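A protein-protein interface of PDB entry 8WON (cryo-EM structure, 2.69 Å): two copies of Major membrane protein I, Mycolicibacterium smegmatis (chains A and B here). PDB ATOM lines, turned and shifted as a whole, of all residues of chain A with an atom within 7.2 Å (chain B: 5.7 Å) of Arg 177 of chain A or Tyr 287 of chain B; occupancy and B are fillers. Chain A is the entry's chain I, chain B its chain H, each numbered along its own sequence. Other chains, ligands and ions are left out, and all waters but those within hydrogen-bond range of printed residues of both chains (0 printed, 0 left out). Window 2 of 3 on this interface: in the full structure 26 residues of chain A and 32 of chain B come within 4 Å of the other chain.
OE2 of Glu 173 of chain A lies within salt-bridge range of NH2 of Arg 177 of chain A. NE2 of His 285 of chain A lies within hydrogen-bond range of OE2 of Glu 173 of chain A, at 3.3 Å.
Arg 172 of chain B touches Asp 144 of chain A. CD of Arg 177 of chain A touches CG2 of Thr 175 of chain B (3.96 Å). CG of Tyr 287 of chain B touches NH2 of Arg 177 of chain A, at 3.7 Å. His 285 of chain A touches Gln 288 of chain B.
Of chain B, only Thr 175 (3.96 Å) and Tyr 287 (3.7 Å) come within 4 Å of Arg 177 of chain A. Tyr 287 of chain B touches one residue of chain A. Of the printed residues of chain A, Arg 172 of chain B touches Asp 144 (3.5 Å). Printed residues of chain A within 4 Å of Thr 175 of chain B: Arg 177. Printed residues of chain B within 4 Å of Asp 144 of chain A: Arg 172 (3.5 Å). Of the printed residues of chain A, Gln 288 of chain B touches His 285. Printed residues of chain B within 4 Å of His 285 of chain A: Gln 288. Pro 143 of chain A touches none of the printed residues of chain B. The nearest printed residue of chain B that does not touch His 285 of chain A is Tyr 287 of chain B (6.2 Å).
Printed residues of chain B that touch a printed residue of chain A: Arg 172, Thr 175, Tyr 287 and Gln 288. Printed residues of chain A that touch a printed residue of chain B: Asp 144, Arg 177 and His 285. Among the printed residues, 4 pairs touch across the chains.
6 positions are printed for both chains. Of the 4 pairs that touch across the chains among the printed residues, none has its exchanged pair printed and touching as well.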
ATOM      1  N   ALA A 140     -30.055   7.343  14.508  1.00  0.00           N
ATOM      2  CA  ALA A 140     -30.613   8.679  14.377  1.00  0.00           C
ATOM      3  C   ALA A 140     -31.113   8.926  12.955  1.00  0.00           C
ATOM      4  O   ALA A 140     -30.545   8.406  11.992  1.00  0.00           O
ATOM      5  CB  ALA A 140     -29.568   9.723  14.746  1.00  0.00           C
ATOM      6  N   PRO A 141     -32.174   9.722  12.795  1.00  0.00           N
ATOM      7  CA  PRO A 141     -32.720   9.990  11.457  1.00  0.00           C
ATOM      8  C   PRO A 141     -31.851  10.980  10.697  1.00  0.00           C
ATOM      9  O   PRO A 141     -31.841  12.178  10.993  1.00  0.00           O
ATOM     10  CB  PRO A 141     -34.109  10.566  11.762  1.00  0.00           C
ATOM     11  CG  PRO A 141     -33.959  11.204  13.081  1.00  0.00           C
ATOM     12  CD  PRO A 141     -32.940  10.408  13.849  1.00  0.00           C
ATOM     13  N   THR A 142     -31.128  10.484   9.714  1.00  0.00           N
ATOM     14  CA  THR A 142     -30.234  11.293   8.904  1.00  0.00           C
ATOM     15  C   THR A 142     -30.847  11.555   7.541  1.00  0.00           C
ATOM     16  O   THR A 142     -31.854  10.951   7.167  1.00  0.00           O
ATOM     17  CB  THR A 142     -28.882  10.599   8.766  1.00  0.00           C
ATOM     18  OG1 THR A 142     -29.037   9.385   8.025  1.00  0.00           O
ATOM     19  CG2 THR A 142     -28.310  10.285  10.131  1.00  0.00           C
ATOM     20  N   PRO A 143     -30.283  12.495   6.778  1.00  0.00           N
ATOM     21  CA  PRO A 143     -30.765  12.711   5.403  1.00  0.00           C
ATOM     22  C   PRO A 143     -30.716  11.482   4.505  1.00  0.00           C
ATOM     23  O   PRO A 143     -31.548  11.365   3.599  1.00  0.00           O
ATOM     24  CB  PRO A 143     -29.838  13.821   4.901  1.00  0.00           C
ATOM     25  CG  PRO A 143     -29.518  14.598   6.118  1.00  0.00           C
ATOM     26  CD  PRO A 143     -29.448  13.617   7.248  1.00  0.00           C
ATOM     27  N   ASP A 144     -29.771  10.563   4.719  1.00  0.00           N
ATOM     28  CA  ASP A 144     -29.731   9.336   3.924  1.00  0.00           C
ATOM     29  C   ASP A 144     -30.972   8.479   4.140  1.00  0.00           C
ATOM     30  O   ASP A 144     -31.515   7.907   3.189  1.00  0.00           O
ATOM     31  CB  ASP A 144     -28.479   8.533   4.260  1.00  0.00           C
ATOM     32  CG  ASP A 144     -27.208   9.261   3.908  1.00  0.00           C
ATOM     33  OD1 ASP A 144     -27.288  10.430   3.478  1.00  0.00           O
ATOM     34  OD2 ASP A 144     -26.123   8.667   4.069  1.00  0.00           O
ATOM     35  N   PHE A 170     -34.132  15.007  13.562  1.00  0.00           N
ATOM     36  CA  PHE A 170     -33.755  15.212  12.170  1.00  0.00           C
ATOM     37  C   PHE A 170     -33.084  16.563  11.970  1.00  0.00           C
ATOM     38  O   PHE A 170     -32.100  16.667  11.230  1.00  0.00           O
ATOM     39  CB  PHE A 170     -34.977  15.091  11.265  1.00  0.00           C
ATOM     40  CG  PHE A 170     -34.672  15.337   9.822  1.00  0.00           C
ATOM     41  CD1 PHE A 170     -33.858  14.469   9.117  1.00  0.00           C
ATOM     42  CD2 PHE A 170     -35.175  16.448   9.175  1.00  0.00           C
ATOM     43  CE1 PHE A 170     -33.565  14.695   7.794  1.00  0.00           C
ATOM     44  CE2 PHE A 170     -34.884  16.678   7.847  1.00  0.00           C
ATOM     45  CZ  PHE A 170     -34.078  15.798   7.157  1.00  0.00           C
ATOM     46  N   GLY A 171     -33.613  17.614  12.602  1.00  0.00           N
ATOM     47  CA  GLY A 171     -32.984  18.918  12.493  1.00  0.00           C
ATOM     48  C   GLY A 171     -31.570  18.932  13.033  1.00  0.00           C
ATOM     49  O   GLY A 171     -30.679  19.554  12.452  1.00  0.00           O
ATOM     50  N   ARG A 172     -31.344  18.249  14.154  1.00  0.00           N
ATOM     51  CA  ARG A 172     -29.994  18.153  14.700  1.00  0.00           C
ATOM     52  C   ARG A 172     -29.054  17.452  13.733  1.00  0.00           C
ATOM     53  O   ARG A 172     -27.927  17.915  13.504  1.00  0.00           O
ATOM     54  CB  ARG A 172     -30.014  17.419  16.035  1.00  0.00           C
ATOM     55  CG  ARG A 172     -30.595  18.212  17.166  1.00  0.00           C
ATOM     56  CD  ARG A 172     -30.165  17.643  18.491  1.00  0.00           C
ATOM     57  NE  ARG A 172     -30.483  16.228  18.634  1.00  0.00           N
ATOM     58  CZ  ARG A 172     -31.656  15.759  19.030  1.00  0.00           C
ATOM     59  NH1 ARG A 172     -32.668  16.565  19.289  1.00  0.00           N
ATOM     60  NH2 ARG A 172     -31.814  14.452  19.178  1.00  0.00           N
ATOM     61  N   GLU A 173     -29.494  16.328  13.162  1.00  0.00           N
ATOM     62  CA  GLU A 173     -28.630  15.596  12.244  1.00  0.00           C
ATOM     63  C   GLU A 173     -28.347  16.406  10.986  1.00  0.00           C
ATOM     64  O   GLU A 173     -27.251  16.328  10.422  1.00  0.00           O
ATOM     65  CB  GLU A 173     -29.247  14.245  11.888  1.00  0.00           C
ATOM     66  CG  GLU A 173     -28.996  13.151  12.917  1.00  0.00           C
ATOM     67  CD  GLU A 173     -27.536  12.724  13.018  1.00  0.00           C
ATOM     68  OE1 GLU A 173     -27.242  11.816  13.820  1.00  0.00           O
ATOM     69  OE2 GLU A 173     -26.680  13.276  12.304  1.00  0.00           O
ATOM     70  N   CYS A 174     -29.327  17.184  10.529  1.00  0.00           N
ATOM     71  CA  CYS A 174     -29.107  18.055   9.380  1.00  0.00           C
ATOM     72  C   CYS A 174     -28.123  19.171   9.702  1.00  0.00           C
ATOM     73  O   CYS A 174     -27.300  19.538   8.860  1.00  0.00           O
ATOM     74  CB  CYS A 174     -30.434  18.638   8.904  1.00  0.00           C
ATOM     75  SG  CYS A 174     -31.319  17.596   7.755  1.00  0.00           S
ATOM     76  N   THR A 175     -28.204  19.739  10.904  1.00  0.00           N
ATOM     77  CA  THR A 175     -27.278  20.800  11.285  1.00  0.00           C
ATOM     78  C   THR A 175     -25.850  20.279  11.405  1.00  0.00           C
ATOM     79  O   THR A 175     -24.901  20.965  11.013  1.00  0.00           O
ATOM     80  CB  THR A 175     -27.738  21.458  12.588  1.00  0.00           C
ATOM     81  OG1 THR A 175     -28.867  22.298  12.322  1.00  0.00           O
ATOM     82  CG2 THR A 175     -26.641  22.304  13.196  1.00  0.00           C
ATOM     83  N   TYR A 176     -25.670  19.068  11.938  1.00  0.00           N
ATOM     84  CA  TYR A 176     -24.319  18.522  12.032  1.00  0.00           C
ATOM     85  C   TYR A 176     -23.692  18.325  10.661  1.00  0.00           C
ATOM     86  O   TYR A 176     -22.476  18.455  10.508  1.00  0.00           O
ATOM     87  CB  TYR A 176     -24.324  17.195  12.774  1.00  0.00           C
ATOM     88  CG  TYR A 176     -22.974  16.526  12.802  1.00  0.00           C
ATOM     89  CD1 TYR A 176     -21.949  17.034  13.577  1.00  0.00           C
ATOM     90  CD2 TYR A 176     -22.723  15.388  12.055  1.00  0.00           C
ATOM     91  CE1 TYR A 176     -20.719  16.432  13.613  1.00  0.00           C
ATOM     92  CE2 TYR A 176     -21.493  14.779  12.080  1.00  0.00           C
ATOM     93  CZ  TYR A 176     -20.492  15.308  12.863  1.00  0.00           C
ATOM     94  OH  TYR A 176     -19.258  14.709  12.901  1.00  0.00           O
ATOM     95  N   ARG A 177     -24.500  18.001   9.659  1.00  0.00           N
ATOM     96  CA  ARG A 177     -24.003  17.793   8.310  1.00  0.00           C
ATOM     97  C   ARG A 177     -23.847  19.090   7.535  1.00  0.00           C
ATOM     98  O   ARG A 177     -23.411  19.051   6.383  1.00  0.00           O
ATOM     99  CB  ARG A 177     -24.933  16.843   7.556  1.00  0.00           C
ATOM    100  CG  ARG A 177     -24.513  15.397   7.635  1.00  0.00           C
ATOM    101  CD  ARG A 177     -25.704  14.466   7.651  1.00  0.00           C
ATOM    102  NE  ARG A 177     -25.372  13.181   8.250  1.00  0.00           N
ATOM    103  CZ  ARG A 177     -25.298  12.958   9.553  1.00  0.00           C
ATOM    104  NH1 ARG A 177     -25.569  13.906  10.431  1.00  0.00           N
ATOM    105  NH2 ARG A 177     -24.942  11.755   9.985  1.00  0.00           N
ATOM    106  N   GLY A 178     -24.186  20.228   8.133  1.00  0.00           N
ATOM    107  CA  GLY A 178     -24.046  21.501   7.465  1.00  0.00           C
ATOM    108  C   GLY A 178     -25.113  21.808   6.449  1.00  0.00           C
ATOM    109  O   GLY A 178     -24.891  22.643   5.570  1.00  0.00           O
ATOM    110  N   VAL A 179     -26.270  21.161   6.540  1.00  0.00           N
ATOM    111  CA  VAL A 179     -27.341  21.335   5.563  1.00  0.00           C
ATOM    112  C   VAL A 179     -28.566  21.926   6.248  1.00  0.00           C
ATOM    113  O   VAL A 179     -29.199  21.253   7.071  1.00  0.00           O
ATOM    114  CB  VAL A 179     -27.680  19.998   4.881  1.00  0.00           C
ATOM    115  CG1 VAL A 179     -28.992  20.104   4.135  1.00  0.00           C
ATOM    116  CG2 VAL A 179     -26.556  19.583   3.945  1.00  0.00           C
ATOM    117  N   PRO A 180     -28.917  23.179   5.980  1.00  0.00           N
ATOM    118  CA  PRO A 180     -30.161  23.736   6.518  1.00  0.00           C
ATOM    119  C   PRO A 180     -31.337  23.470   5.592  1.00  0.00           C
ATOM    120  O   PRO A 180     -31.349  23.934   4.442  1.00  0.00           O
ATOM    121  CB  PRO A 180     -29.855  25.237   6.620  1.00  0.00           C
ATOM    122  CG  PRO A 180     -28.833  25.483   5.572  1.00  0.00           C
ATOM    123  CD  PRO A 180     -28.077  24.205   5.337  1.00  0.00           C
ATOM    124  N   HIS A 285     -24.496  15.562  19.132  1.00  0.00           N
ATOM    125  CA  HIS A 285     -23.132  15.657  18.640  1.00  0.00           C
ATOM    126  C   HIS A 285     -22.324  16.611  19.507  1.00  0.00           C
ATOM    127  O   HIS A 285     -22.860  17.551  20.096  1.00  0.00           O
ATOM    128  CB  HIS A 285     -23.105  16.135  17.187  1.00  0.00           C
ATOM    129  CG  HIS A 285     -23.527  15.093  16.201  1.00  0.00           C
ATOM    130  ND1 HIS A 285     -22.785  13.957  15.956  1.00  0.00           N
ATOM    131  CD2 HIS A 285     -24.608  15.019  15.390  1.00  0.00           C
ATOM    132  CE1 HIS A 285     -23.398  13.226  15.044  1.00  0.00           C
ATOM    133  NE2 HIS A 285     -24.503  13.850  14.683  1.00  0.00           N
ATOM    134  N   TYR A 287     -19.173  19.411  20.079  1.00  0.00           N
ATOM    135  CA  TYR A 287     -18.714  20.603  19.381  1.00  0.00           C
ATOM    136  C   TYR A 287     -17.656  21.276  20.252  1.00  0.00           C
ATOM    137  O   TYR A 287     -17.061  20.632  21.122  1.00  0.00           O
ATOM    138  CB  TYR A 287     -19.896  21.535  19.062  1.00  0.00           C
ATOM    139  CG  TYR A 287     -20.845  21.039  17.997  1.00  0.00           C
ATOM    140  CD1 TYR A 287     -20.555  21.202  16.650  1.00  0.00           C
ATOM    141  CD2 TYR A 287     -22.052  20.445  18.335  1.00  0.00           C
ATOM    142  CE1 TYR A 287     -21.427  20.769  15.676  1.00  0.00           C
ATOM    143  CE2 TYR A 287     -22.928  20.014  17.370  1.00  0.00           C
ATOM    144  CZ  TYR A 287     -22.612  20.178  16.043  1.00  0.00           C
ATOM    145  OH  TYR A 287     -23.486  19.749  15.081  1.00  0.00           O
ATOM    146  N   ARG B 172     -27.029  11.785  -1.514  1.00  0.00           N
ATOM    147  CA  ARG B 172     -26.059  11.419  -0.486  1.00  0.00           C
ATOM    148  C   ARG B 172     -24.712  12.076  -0.734  1.00  0.00           C
ATOM    149  O   ARG B 172     -24.097  12.621   0.193  1.00  0.00           O
ATOM    150  CB  ARG B 172     -25.900   9.904  -0.427  1.00  0.00           C
ATOM    151  CG  ARG B 172     -27.064   9.185   0.181  1.00  0.00           C
ATOM    152  CD  ARG B 172     -26.663   7.807   0.634  1.00  0.00           C
ATOM    153  NE  ARG B 172     -26.058   7.012  -0.429  1.00  0.00           N
ATOM    154  CZ  ARG B 172     -26.741   6.313  -1.322  1.00  0.00           C
ATOM    155  NH1 ARG B 172     -28.060   6.320  -1.342  1.00  0.00           N
ATOM    156  NH2 ARG B 172     -26.084   5.579  -2.208  1.00  0.00           N
ATOM    157  N   THR B 175     -24.894  15.705   0.127  1.00  0.00           N
ATOM    158  CA  THR B 175     -24.927  15.951   1.566  1.00  0.00           C
ATOM    159  C   THR B 175     -23.547  15.784   2.192  1.00  0.00           C
ATOM    160  O   THR B 175     -23.170  16.552   3.084  1.00  0.00           O
ATOM    161  CB  THR B 175     -25.953  15.035   2.232  1.00  0.00           C
ATOM    162  OG1 THR B 175     -27.272  15.509   1.942  1.00  0.00           O
ATOM    163  CG2 THR B 175     -25.770  15.002   3.733  1.00  0.00           C
ATOM    164  N   TYR B 176     -22.773  14.793   1.743  1.00  0.00           N
ATOM    165  CA  TYR B 176     -21.431  14.627   2.294  1.00  0.00           C
ATOM    166  C   TYR B 176     -20.549  15.832   2.005  1.00  0.00           C
ATOM    167  O   TYR B 176     -19.674  16.171   2.807  1.00  0.00           O
ATOM    168  CB  TYR B 176     -20.768  13.378   1.736  1.00  0.00           C
ATOM    169  CG  TYR B 176     -19.338  13.217   2.181  1.00  0.00           C
ATOM    170  CD1 TYR B 176     -19.037  12.878   3.485  1.00  0.00           C
ATOM    171  CD2 TYR B 176     -18.288  13.403   1.297  1.00  0.00           C
ATOM    172  CE1 TYR B 176     -17.739  12.724   3.900  1.00  0.00           C
ATOM    173  CE2 TYR B 176     -16.985  13.257   1.702  1.00  0.00           C
ATOM    174  CZ  TYR B 176     -16.716  12.917   3.008  1.00  0.00           C
ATOM    175  OH  TYR B 176     -15.418  12.764   3.428  1.00  0.00           O
ATOM    176  N   GLY B 178     -21.572  18.863   1.880  1.00  0.00           N
ATOM    177  CA  GLY B 178     -22.113  20.040   2.520  1.00  0.00           C
ATOM    178  C   GLY B 178     -22.901  20.951   1.616  1.00  0.00           C
ATOM    179  O   GLY B 178     -23.066  22.129   1.938  1.00  0.00           O
ATOM    180  N   HIS B 285     -21.213   6.989   3.184  1.00  0.00           N
ATOM    181  CA  HIS B 285     -20.135   7.630   3.917  1.00  0.00           C
ATOM    182  C   HIS B 285     -20.293   7.383   5.412  1.00  0.00           C
ATOM    183  O   HIS B 285     -21.403   7.215   5.918  1.00  0.00           O
ATOM    184  CB  HIS B 285     -20.108   9.135   3.647  1.00  0.00           C
ATOM    185  CG  HIS B 285     -19.579   9.498   2.296  1.00  0.00           C
ATOM    186  ND1 HIS B 285     -18.264   9.298   1.935  1.00  0.00           N
ATOM    187  CD2 HIS B 285     -20.184  10.053   1.222  1.00  0.00           C
ATOM    188  CE1 HIS B 285     -18.085   9.708   0.694  1.00  0.00           C
ATOM    189  NE2 HIS B 285     -19.234  10.174   0.240  1.00  0.00           N
ATOM    190  N   GLU B 286     -19.165   7.366   6.113  1.00  0.00           N
ATOM    191  CA  GLU B 286     -19.160   7.175   7.551  1.00  0.00           C
ATOM    192  C   GLU B 286     -19.205   8.519   8.272  1.00  0.00           C
ATOM    193  O   GLU B 286     -18.745   9.540   7.759  1.00  0.00           O
ATOM    194  CB  GLU B 286     -17.928   6.386   7.990  1.00  0.00           C
ATOM    195  CG  GLU B 286     -18.048   4.886   7.774  1.00  0.00           C
ATOM    196  CD  GLU B 286     -19.445   4.359   8.052  1.00  0.00           C
ATOM    197  OE1 GLU B 286     -19.969   4.603   9.161  1.00  0.00           O
ATOM    198  OE2 GLU B 286     -20.022   3.702   7.158  1.00  0.00           O
ATOM    199  N   TYR B 287     -19.753   8.498   9.480  1.00  0.00           N
ATOM    200  CA  TYR B 287     -19.999   9.704  10.260  1.00  0.00           C
ATOM    201  C   TYR B 287     -19.793   9.356  11.732  1.00  0.00           C
ATOM    202  O   TYR B 287     -19.127   8.368  12.054  1.00  0.00           O
ATOM    203  CB  TYR B 287     -21.404  10.261   9.975  1.00  0.00           C
ATOM    204  CG  TYR B 287     -21.596  10.872   8.606  1.00  0.00           C
ATOM    205  CD1 TYR B 287     -21.195  12.172   8.343  1.00  0.00           C
ATOM    206  CD2 TYR B 287     -22.213  10.163   7.587  1.00  0.00           C
ATOM    207  CE1 TYR B 287     -21.387  12.741   7.102  1.00  0.00           C
ATOM    208  CE2 TYR B 287     -22.410  10.722   6.349  1.00  0.00           C
ATOM    209  CZ  TYR B 287     -21.996  12.009   6.111  1.00  0.00           C
ATOM    210  OH  TYR B 287     -22.193  12.569   4.877  1.00  0.00           O
ATOM    211  N   GLN B 288     -20.334  10.190  12.621  1.00  0.00           N
ATOM    212  CA  GLN B 288     -20.251   9.979  14.071  1.00  0.00           C
ATOM    213  C   GLN B 288     -18.815  10.120  14.556  1.00  0.00           C
ATOM    214  O   GLN B 288     -18.384  11.207  14.936  1.00  0.00           O
ATOM    215  CB  GLN B 288     -20.813   8.603  14.457  1.00  0.00           C
ATOM    216  CG  GLN B 288     -21.336   8.461  15.881  1.00  0.00           C
ATOM    217  CD  GLN B 288     -22.206   9.611  16.332  1.00  0.00           C
ATOM    218  OE1 GLN B 288     -23.279   9.845  15.785  1.00  0.00           O
ATOM    219  NE2 GLN B 288     -21.756  10.321  17.359  1.00  0.00           N
